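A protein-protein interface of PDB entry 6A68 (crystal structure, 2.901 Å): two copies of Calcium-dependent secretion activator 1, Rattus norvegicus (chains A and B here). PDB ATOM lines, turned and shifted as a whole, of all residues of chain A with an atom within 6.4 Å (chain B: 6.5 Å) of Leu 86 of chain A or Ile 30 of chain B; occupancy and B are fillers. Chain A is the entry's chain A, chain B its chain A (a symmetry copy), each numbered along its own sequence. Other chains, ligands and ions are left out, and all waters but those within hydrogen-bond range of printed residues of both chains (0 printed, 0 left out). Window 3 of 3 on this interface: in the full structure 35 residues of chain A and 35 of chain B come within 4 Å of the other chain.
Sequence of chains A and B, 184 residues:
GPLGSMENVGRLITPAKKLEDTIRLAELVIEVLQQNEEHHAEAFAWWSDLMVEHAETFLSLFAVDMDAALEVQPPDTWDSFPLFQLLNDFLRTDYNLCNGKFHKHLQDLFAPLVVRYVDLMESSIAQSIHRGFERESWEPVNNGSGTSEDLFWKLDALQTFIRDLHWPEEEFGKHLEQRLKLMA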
ATOM      1  N   LEU A  59      -4.373   7.138 -25.781  1.00  0.00           N
ATOM      2  CA  LEU A  59      -4.326   6.105 -24.758  1.00  0.00           C
ATOM      3  C   LEU A  59      -3.047   6.210 -23.942  1.00  0.00           C
ATOM      4  O   LEU A  59      -3.077   5.951 -22.736  1.00  0.00           O
ATOM      5  CB  LEU A  59      -4.488   4.718 -25.388  1.00  0.00           C
ATOM      6  CG  LEU A  59      -5.931   4.360 -25.791  1.00  0.00           C
ATOM      7  CD1 LEU A  59      -6.024   3.026 -26.518  1.00  0.00           C
ATOM      8  CD2 LEU A  59      -6.847   4.365 -24.592  1.00  0.00           C
ATOM      9  N   PHE A  81      -9.243  -4.251 -10.668  1.00  0.00           N
ATOM     10  CA  PHE A  81      -9.478  -5.217 -11.731  1.00  0.00           C
ATOM     11  C   PHE A  81     -10.631  -4.793 -12.637  1.00  0.00           C
ATOM     12  O   PHE A  81     -10.547  -5.008 -13.851  1.00  0.00           O
ATOM     13  CB  PHE A  81      -9.719  -6.607 -11.144  1.00  0.00           C
ATOM     14  CG  PHE A  81      -8.458  -7.396 -10.963  1.00  0.00           C
ATOM     15  CD1 PHE A  81      -7.475  -7.376 -11.936  1.00  0.00           C
ATOM     16  CD2 PHE A  81      -8.242  -8.140  -9.822  1.00  0.00           C
ATOM     17  CE1 PHE A  81      -6.296  -8.096 -11.776  1.00  0.00           C
ATOM     18  CE2 PHE A  81      -7.068  -8.860  -9.654  1.00  0.00           C
ATOM     19  CZ  PHE A  81      -6.093  -8.836 -10.633  1.00  0.00           C
ATOM     20  N   PRO A  82     -11.710  -4.190 -12.120  1.00  0.00           N
ATOM     21  CA  PRO A  82     -12.734  -3.653 -13.032  1.00  0.00           C
ATOM     22  C   PRO A  82     -12.192  -2.692 -14.080  1.00  0.00           C
ATOM     23  O   PRO A  82     -12.773  -2.592 -15.167  1.00  0.00           O
ATOM     24  CB  PRO A  82     -13.710  -2.952 -12.077  1.00  0.00           C
ATOM     25  CG  PRO A  82     -13.611  -3.704 -10.852  1.00  0.00           C
ATOM     26  CD  PRO A  82     -12.177  -4.133 -10.724  1.00  0.00           C
ATOM     27  N   LEU A  83     -11.106  -1.973 -13.791  1.00  0.00           N
ATOM     28  CA  LEU A  83     -10.484  -1.153 -14.820  1.00  0.00           C
ATOM     29  C   LEU A  83      -9.890  -2.019 -15.916  1.00  0.00           C
ATOM     30  O   LEU A  83     -10.131  -1.782 -17.105  1.00  0.00           O
ATOM     31  CB  LEU A  83      -9.402  -0.265 -14.222  1.00  0.00           C
ATOM     32  CG  LEU A  83      -8.853   0.714 -15.256  1.00  0.00           C
ATOM     33  CD1 LEU A  83      -9.415   2.087 -14.967  1.00  0.00           C
ATOM     34  CD2 LEU A  83      -7.337   0.736 -15.289  1.00  0.00           C
ATOM     35  N   PHE A  84      -9.094  -3.016 -15.542  1.00  0.00           N
ATOM     36  CA  PHE A  84      -8.558  -3.914 -16.555  1.00  0.00           C
ATOM     37  C   PHE A  84      -9.673  -4.570 -17.354  1.00  0.00           C
ATOM     38  O   PHE A  84      -9.543  -4.771 -18.567  1.00  0.00           O
ATOM     39  CB  PHE A  84      -7.687  -4.987 -15.926  1.00  0.00           C
ATOM     40  CG  PHE A  84      -7.188  -5.981 -16.918  1.00  0.00           C
ATOM     41  CD1 PHE A  84      -7.912  -7.123 -17.199  1.00  0.00           C
ATOM     42  CD2 PHE A  84      -6.001  -5.756 -17.595  1.00  0.00           C
ATOM     43  CE1 PHE A  84      -7.453  -8.033 -18.131  1.00  0.00           C
ATOM     44  CE2 PHE A  84      -5.530  -6.666 -18.524  1.00  0.00           C
ATOM     45  CZ  PHE A  84      -6.258  -7.805 -18.794  1.00  0.00           C
ATOM     46  N   GLN A  85     -10.774  -4.932 -16.692  1.00  0.00           N
ATOM     47  CA  GLN A  85     -11.873  -5.574 -17.402  1.00  0.00           C
ATOM     48  C   GLN A  85     -12.439  -4.652 -18.469  1.00  0.00           C
ATOM     49  O   GLN A  85     -12.551  -5.032 -19.637  1.00  0.00           O
ATOM     50  CB  GLN A  85     -12.967  -5.997 -16.420  1.00  0.00           C
ATOM     51  CG  GLN A  85     -12.636  -7.257 -15.622  1.00  0.00           C
ATOM     52  CD  GLN A  85     -13.855  -7.870 -14.961  1.00  0.00           C
ATOM     53  OE1 GLN A  85     -13.867  -8.098 -13.750  1.00  0.00           O
ATOM     54  NE2 GLN A  85     -14.889  -8.143 -15.756  1.00  0.00           N
ATOM     55  N   LEU A  86     -12.786  -3.425 -18.082  1.00  0.00           N
ATOM     56  CA  LEU A  86     -13.337  -2.460 -19.027  1.00  0.00           C
ATOM     57  C   LEU A  86     -12.375  -2.197 -20.179  1.00  0.00           C
ATOM     58  O   LEU A  86     -12.768  -2.205 -21.350  1.00  0.00           O
ATOM     59  CB  LEU A  86     -13.666  -1.164 -18.293  1.00  0.00           C
ATOM     60  CG  LEU A  86     -14.039   0.073 -19.102  1.00  0.00           C
ATOM     61  CD1 LEU A  86     -15.553   0.172 -19.282  1.00  0.00           C
ATOM     62  CD2 LEU A  86     -13.480   1.313 -18.416  1.00  0.00           C
ATOM     63  N   LEU A  87     -11.102  -1.966 -19.867  1.00  0.00           N
ATOM     64  CA  LEU A  87     -10.171  -1.587 -20.919  1.00  0.00           C
ATOM     65  C   LEU A  87      -9.840  -2.766 -21.821  1.00  0.00           C
ATOM     66  O   LEU A  87      -9.792  -2.621 -23.048  1.00  0.00           O
ATOM     67  CB  LEU A  87      -8.903  -0.995 -20.309  1.00  0.00           C
ATOM     68  CG  LEU A  87      -8.936   0.511 -20.038  1.00  0.00           C
ATOM     69  CD1 LEU A  87      -7.547   1.023 -19.772  1.00  0.00           C
ATOM     70  CD2 LEU A  87      -9.536   1.239 -21.211  1.00  0.00           C
ATOM     71  N   ASN A  88      -9.604  -3.937 -21.238  1.00  0.00           N
ATOM     72  CA  ASN A  88      -9.209  -5.085 -22.045  1.00  0.00           C
ATOM     73  C   ASN A  88     -10.385  -5.637 -22.837  1.00  0.00           C
ATOM     74  O   ASN A  88     -10.203  -6.101 -23.966  1.00  0.00           O
ATOM     75  CB  ASN A  88      -8.593  -6.158 -21.147  1.00  0.00           C
ATOM     76  CG  ASN A  88      -8.341  -7.463 -21.871  1.00  0.00           C
ATOM     77  OD1 ASN A  88      -7.428  -7.565 -22.685  1.00  0.00           O
ATOM     78  ND2 ASN A  88      -9.135  -8.480 -21.552  1.00  0.00           N
ATOM     79  N   ASP A  89     -11.597  -5.576 -22.283  1.00  0.00           N
ATOM     80  CA  ASP A  89     -12.757  -6.057 -23.023  1.00  0.00           C
ATOM     81  C   ASP A  89     -13.026  -5.205 -24.258  1.00  0.00           C
ATOM     82  O   ASP A  89     -13.597  -5.698 -25.235  1.00  0.00           O
ATOM     83  CB  ASP A  89     -13.990  -6.090 -22.118  1.00  0.00           C
ATOM     84  CG  ASP A  89     -14.154  -7.418 -21.394  1.00  0.00           C
ATOM     85  OD1 ASP A  89     -13.305  -8.314 -21.584  1.00  0.00           O
ATOM     86  OD2 ASP A  89     -15.144  -7.564 -20.645  1.00  0.00           O
ATOM     87  N   PHE A  90     -12.636  -3.927 -24.234  1.00  0.00           N
ATOM     88  CA  PHE A  90     -12.742  -3.086 -25.420  1.00  0.00           C
ATOM     89  C   PHE A  90     -11.628  -3.398 -26.412  1.00  0.00           C
ATOM     90  O   PHE A  90     -11.885  -3.663 -27.591  1.00  0.00           O
ATOM     91  CB  PHE A  90     -12.717  -1.606 -25.016  1.00  0.00           C
ATOM     92  CG  PHE A  90     -12.278  -0.665 -26.119  1.00  0.00           C
ATOM     93  CD1 PHE A  90     -13.171  -0.240 -27.090  1.00  0.00           C
ATOM     94  CD2 PHE A  90     -10.977  -0.184 -26.168  1.00  0.00           C
ATOM     95  CE1 PHE A  90     -12.766   0.624 -28.098  1.00  0.00           C
ATOM     96  CE2 PHE A  90     -10.568   0.676 -27.179  1.00  0.00           C
ATOM     97  CZ  PHE A  90     -11.461   1.083 -28.139  1.00  0.00           C
ATOM     98  N   LEU A  91     -10.383  -3.394 -25.940  1.00  0.00           N
ATOM     99  CA  LEU A  91      -9.238  -3.518 -26.836  1.00  0.00           C
ATOM    100  C   LEU A  91      -9.188  -4.871 -27.542  1.00  0.00           C
ATOM    101  O   LEU A  91      -8.704  -4.952 -28.678  1.00  0.00           O
ATOM    102  CB  LEU A  91      -7.941  -3.293 -26.055  1.00  0.00           C
ATOM    103  CG  LEU A  91      -7.649  -1.883 -25.554  1.00  0.00           C
ATOM    104  CD1 LEU A  91      -6.555  -1.904 -24.511  1.00  0.00           C
ATOM    105  CD2 LEU A  91      -7.236  -1.021 -26.719  1.00  0.00           C
ATOM    106  N   THR B  22      -9.986   7.570 -12.437  1.00  0.00           N
ATOM    107  CA  THR B  22      -9.372   6.917 -13.590  1.00  0.00           C
ATOM    108  C   THR B  22     -10.375   6.056 -14.355  1.00  0.00           C
ATOM    109  O   THR B  22     -10.304   5.972 -15.586  1.00  0.00           O
ATOM    110  CB  THR B  22      -8.176   6.080 -13.136  1.00  0.00           C
ATOM    111  OG1 THR B  22      -7.145   6.954 -12.664  1.00  0.00           O
ATOM    112  CG2 THR B  22      -7.616   5.245 -14.282  1.00  0.00           C
ATOM    113  N   ILE B  23     -11.321   5.426 -13.653  1.00  0.00           N
ATOM    114  CA  ILE B  23     -12.350   4.627 -14.319  1.00  0.00           C
ATOM    115  C   ILE B  23     -13.187   5.506 -15.241  1.00  0.00           C
ATOM    116  O   ILE B  23     -13.239   5.286 -16.454  1.00  0.00           O
ATOM    117  CB  ILE B  23     -13.243   3.908 -13.289  1.00  0.00           C
ATOM    118  CG1 ILE B  23     -12.503   2.790 -12.532  1.00  0.00           C
ATOM    119  CG2 ILE B  23     -14.506   3.376 -13.968  1.00  0.00           C
ATOM    120  CD1 ILE B  23     -12.452   1.475 -13.238  1.00  0.00           C
ATOM    121  N   ARG B  24     -13.852   6.519 -14.674  1.00  0.00           N
ATOM    122  CA  ARG B  24     -14.750   7.358 -15.465  1.00  0.00           C
ATOM    123  C   ARG B  24     -14.031   7.983 -16.654  1.00  0.00           C
ATOM    124  O   ARG B  24     -14.642   8.196 -17.706  1.00  0.00           O
ATOM    125  CB  ARG B  24     -15.375   8.444 -14.579  1.00  0.00           C
ATOM    126  CG  ARG B  24     -16.509   7.945 -13.676  1.00  0.00           C
ATOM    127  CD  ARG B  24     -17.103   9.067 -12.835  1.00  0.00           C
ATOM    128  N   LEU B  25     -12.738   8.268 -16.516  1.00  0.00           N
ATOM    129  CA  LEU B  25     -11.978   8.782 -17.648  1.00  0.00           C
ATOM    130  C   LEU B  25     -11.798   7.708 -18.710  1.00  0.00           C
ATOM    131  O   LEU B  25     -11.988   7.968 -19.905  1.00  0.00           O
ATOM    132  CB  LEU B  25     -10.618   9.304 -17.179  1.00  0.00           C
ATOM    133  CG  LEU B  25      -9.794   9.946 -18.295  1.00  0.00           C
ATOM    134  CD1 LEU B  25     -10.294  11.355 -18.562  1.00  0.00           C
ATOM    135  CD2 LEU B  25      -8.308   9.945 -17.987  1.00  0.00           C
ATOM    136  N   ALA B  26     -11.413   6.495 -18.297  1.00  0.00           N
ATOM    137  CA  ALA B  26     -11.325   5.383 -19.237  1.00  0.00           C
ATOM    138  C   ALA B  26     -12.654   5.157 -19.946  1.00  0.00           C
ATOM    139  O   ALA B  26     -12.692   4.935 -21.158  1.00  0.00           O
ATOM    140  CB  ALA B  26     -10.888   4.113 -18.513  1.00  0.00           C
ATOM    141  N   GLU B  27     -13.756   5.227 -19.206  1.00  0.00           N
ATOM    142  CA  GLU B  27     -15.069   5.163 -19.830  1.00  0.00           C
ATOM    143  C   GLU B  27     -15.198   6.177 -20.966  1.00  0.00           C
ATOM    144  O   GLU B  27     -15.724   5.857 -22.038  1.00  0.00           O
ATOM    145  CB  GLU B  27     -16.153   5.393 -18.774  1.00  0.00           C
ATOM    146  CG  GLU B  27     -16.444   4.188 -17.884  1.00  0.00           C
ATOM    147  CD  GLU B  27     -17.683   4.395 -17.024  1.00  0.00           C
ATOM    148  OE1 GLU B  27     -18.003   5.566 -16.720  1.00  0.00           O
ATOM    149  OE2 GLU B  27     -18.342   3.393 -16.658  1.00  0.00           O
ATOM    150  N   LEU B  28     -14.711   7.405 -20.755  1.00  0.00           N
ATOM    151  CA  LEU B  28     -14.877   8.449 -21.762  1.00  0.00           C
ATOM    152  C   LEU B  28     -13.906   8.279 -22.927  1.00  0.00           C
ATOM    153  O   LEU B  28     -14.280   8.494 -24.083  1.00  0.00           O
ATOM    154  CB  LEU B  28     -14.709   9.830 -21.131  1.00  0.00           C
ATOM    155  CG  LEU B  28     -14.608  10.955 -22.163  1.00  0.00           C
ATOM    156  CD1 LEU B  28     -15.983  11.522 -22.485  1.00  0.00           C
ATOM    157  CD2 LEU B  28     -13.652  12.056 -21.722  1.00  0.00           C
ATOM    158  N   VAL B  29     -12.661   7.902 -22.652  1.00  0.00           N
ATOM    159  CA  VAL B  29     -11.730   7.639 -23.743  1.00  0.00           C
ATOM    160  C   VAL B  29     -12.276   6.548 -24.646  1.00  0.00           C
ATOM    161  O   VAL B  29     -12.292   6.682 -25.871  1.00  0.00           O
ATOM    162  CB  VAL B  29     -10.350   7.263 -23.191  1.00  0.00           C
ATOM    163  CG1 VAL B  29      -9.477   6.716 -24.309  1.00  0.00           C
ATOM    164  CG2 VAL B  29      -9.717   8.470 -22.521  1.00  0.00           C
ATOM    165  N   ILE B  30     -12.735   5.447 -24.049  1.00  0.00           N
ATOM    166  CA  ILE B  30     -13.302   4.349 -24.827  1.00  0.00           C
ATOM    167  C   ILE B  30     -14.447   4.849 -25.695  1.00  0.00           C
ATOM    168  O   ILE B  30     -14.498   4.570 -26.896  1.00  0.00           O
ATOM    169  CB  ILE B  30     -13.758   3.212 -23.897  1.00  0.00           C
ATOM    170  CG1 ILE B  30     -12.563   2.396 -23.438  1.00  0.00           C
ATOM    171  CG2 ILE B  30     -14.740   2.303 -24.586  1.00  0.00           C
ATOM    172  CD1 ILE B  30     -12.894   1.502 -22.284  1.00  0.00           C
ATOM    173  N   GLU B  31     -15.372   5.617 -25.111  1.00  0.00           N
ATOM    174  CA  GLU B  31     -16.540   6.047 -25.872  1.00  0.00           C
ATOM    175  C   GLU B  31     -16.138   6.927 -27.052  1.00  0.00           C
ATOM    176  O   GLU B  31     -16.612   6.720 -28.174  1.00  0.00           O
ATOM    177  CB  GLU B  31     -17.543   6.770 -24.969  1.00  0.00           C
ATOM    178  CG  GLU B  31     -18.341   7.862 -25.679  1.00  0.00           C
ATOM    179  CD  GLU B  31     -19.479   8.430 -24.826  1.00  0.00           C
ATOM    180  OE1 GLU B  31     -20.523   7.747 -24.688  1.00  0.00           O
ATOM    181  OE2 GLU B  31     -19.343   9.572 -24.322  1.00  0.00           O
ATOM    182  N   VAL B  32     -15.245   7.889 -26.838  1.00  0.00           N
ATOM    183  CA  VAL B  32     -14.761   8.703 -27.949  1.00  0.00           C
ATOM    184  C   VAL B  32     -14.081   7.824 -28.999  1.00  0.00           C
ATOM    185  O   VAL B  32     -14.338   7.943 -30.200  1.00  0.00           O
ATOM    186  CB  VAL B  32     -13.824   9.810 -27.431  1.00  0.00           C
ATOM    187  CG1 VAL B  32     -12.861  10.263 -28.511  1.00  0.00           C
ATOM    188  CG2 VAL B  32     -14.649  10.971 -26.917  1.00  0.00           C
ATOM    189  N   LEU B  33     -13.218   6.916 -28.555  1.00  0.00           N
ATOM    190  CA  LEU B  33     -12.466   6.089 -29.493  1.00  0.00           C
ATOM    191  C   LEU B  33     -13.387   5.226 -30.341  1.00  0.00           C
ATOM    192  O   LEU B  33     -13.101   4.977 -31.516  1.00  0.00           O
ATOM    193  CB  LEU B  33     -11.473   5.209 -28.738  1.00  0.00           C
ATOM    194  CG  LEU B  33     -10.340   5.916 -28.014  1.00  0.00           C
ATOM    195  CD1 LEU B  33      -9.142   4.994 -27.937  1.00  0.00           C
ATOM    196  CD2 LEU B  33      -9.992   7.199 -28.711  1.00  0.00           C
ATOM    197  N   GLN B  34     -14.486   4.744 -29.756  1.00  0.00           N
ATOM    198  CA  GLN B  34     -15.443   3.923 -30.490  1.00  0.00           C
ATOM    199  C   GLN B  34     -16.265   4.763 -31.457  1.00  0.00           C
ATOM    200  O   GLN B  34     -16.425   4.405 -32.630  1.00  0.00           O
ATOM    201  CB  GLN B  34     -16.370   3.213 -29.511  1.00  0.00           C
ATOM    202  CG  GLN B  34     -15.757   2.032 -28.826  1.00  0.00           C
ATOM    203  CD  GLN B  34     -16.764   1.281 -27.991  1.00  0.00           C
ATOM    204  OE1 GLN B  34     -17.631   1.884 -27.340  1.00  0.00           O
ATOM    205  NE2 GLN B  34     -16.658  -0.048 -28.000  1.00  0.00           N
ATOM    206  N   GLN B  35     -16.836   5.860 -30.956  1.00  0.00           N
ATOM    207  CA  GLN B  35     -17.496   6.842 -31.804  1.00  0.00           C
ATOM    208  C   GLN B  35     -16.658   7.177 -33.037  1.00  0.00           C
ATOM    209  O   GLN B  35     -17.194   7.327 -34.140  1.00  0.00           O
ATOM    210  CB  GLN B  35     -17.775   8.086 -30.971  1.00  0.00           C
ATOM    211  CG  GLN B  35     -18.668   9.111 -31.615  1.00  0.00           C
ATOM    212  CD  GLN B  35     -18.642  10.423 -30.851  1.00  0.00           C
ATOM    213  OE1 GLN B  35     -18.296  10.451 -29.663  1.00  0.00           O
ATOM    214  NE2 GLN B  35     -18.992  11.524 -31.530  1.00  0.00           N
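CD2 of Leu 59 of chain A touches CG1 of Val 29 of chain B, 3.5 Å away.
Leu 59 of chain A touches Leu 33 of chain B.
Leu 83 of chain A touches Thr 22 of chain B (CD1 to CG2, 3.7 Å).
Ile 23 of chain B touches Leu 83 of chain A.
CD2 of Leu 86 of chain A touches CB of Ala 26 of chain B (3.8 Å).
CG of Leu 86 of chain A touches CD1 of Ile 30 of chain B, at 3.7 Å.
Leu 87 of chain A touches Ile 30 of chain B.
Phe 90 of chain A touches Ile 30 of chain B.
CE1 of Phe 90 of chain A touches CG of Gln 34 of chain B, at 3.4 Å.
No position is printed for both chains.
Of the 9 pairs that touch across the chains among the printed residues, none has its exchanged pair printed and touching as well.
Hydrophobic or aromatic side chains of chain A within 4 Å of the printed part of chain B: Leu 59, Leu 83, Leu 86, Leu 87 and Phe 90.
Of the 14 printed residues of chain B, 7 touch a printed residue of chain A.
Hydrophobic or aromatic side chains of chain B within 4 Å of the printed part of chain A: Ile 23, Ala 26, Val 29, Ile 30 and Leu 33.
Among the printed residues, 9 pairs touch across the chains.
Among the printed residues, no Asp or Glu carboxylate lies within 4 Å of a Lys or Arg side-chain nitrogen of the other chain.
Of the printed residues of chain B, Leu 83 of chain A touches Thr 22 (3.7 Å) and Ile 23 (3.5 Å).
Printed residues of chain B within 4 Å of Leu 86 of chain A: Ala 26 and Ile 30.
Printed residues of chain B within 4 Å of Leu 87 of chain A: Ile 30.
Of the printed residues of chain A, Val 29 of chain B touches Leu 59 (3.5 Å).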
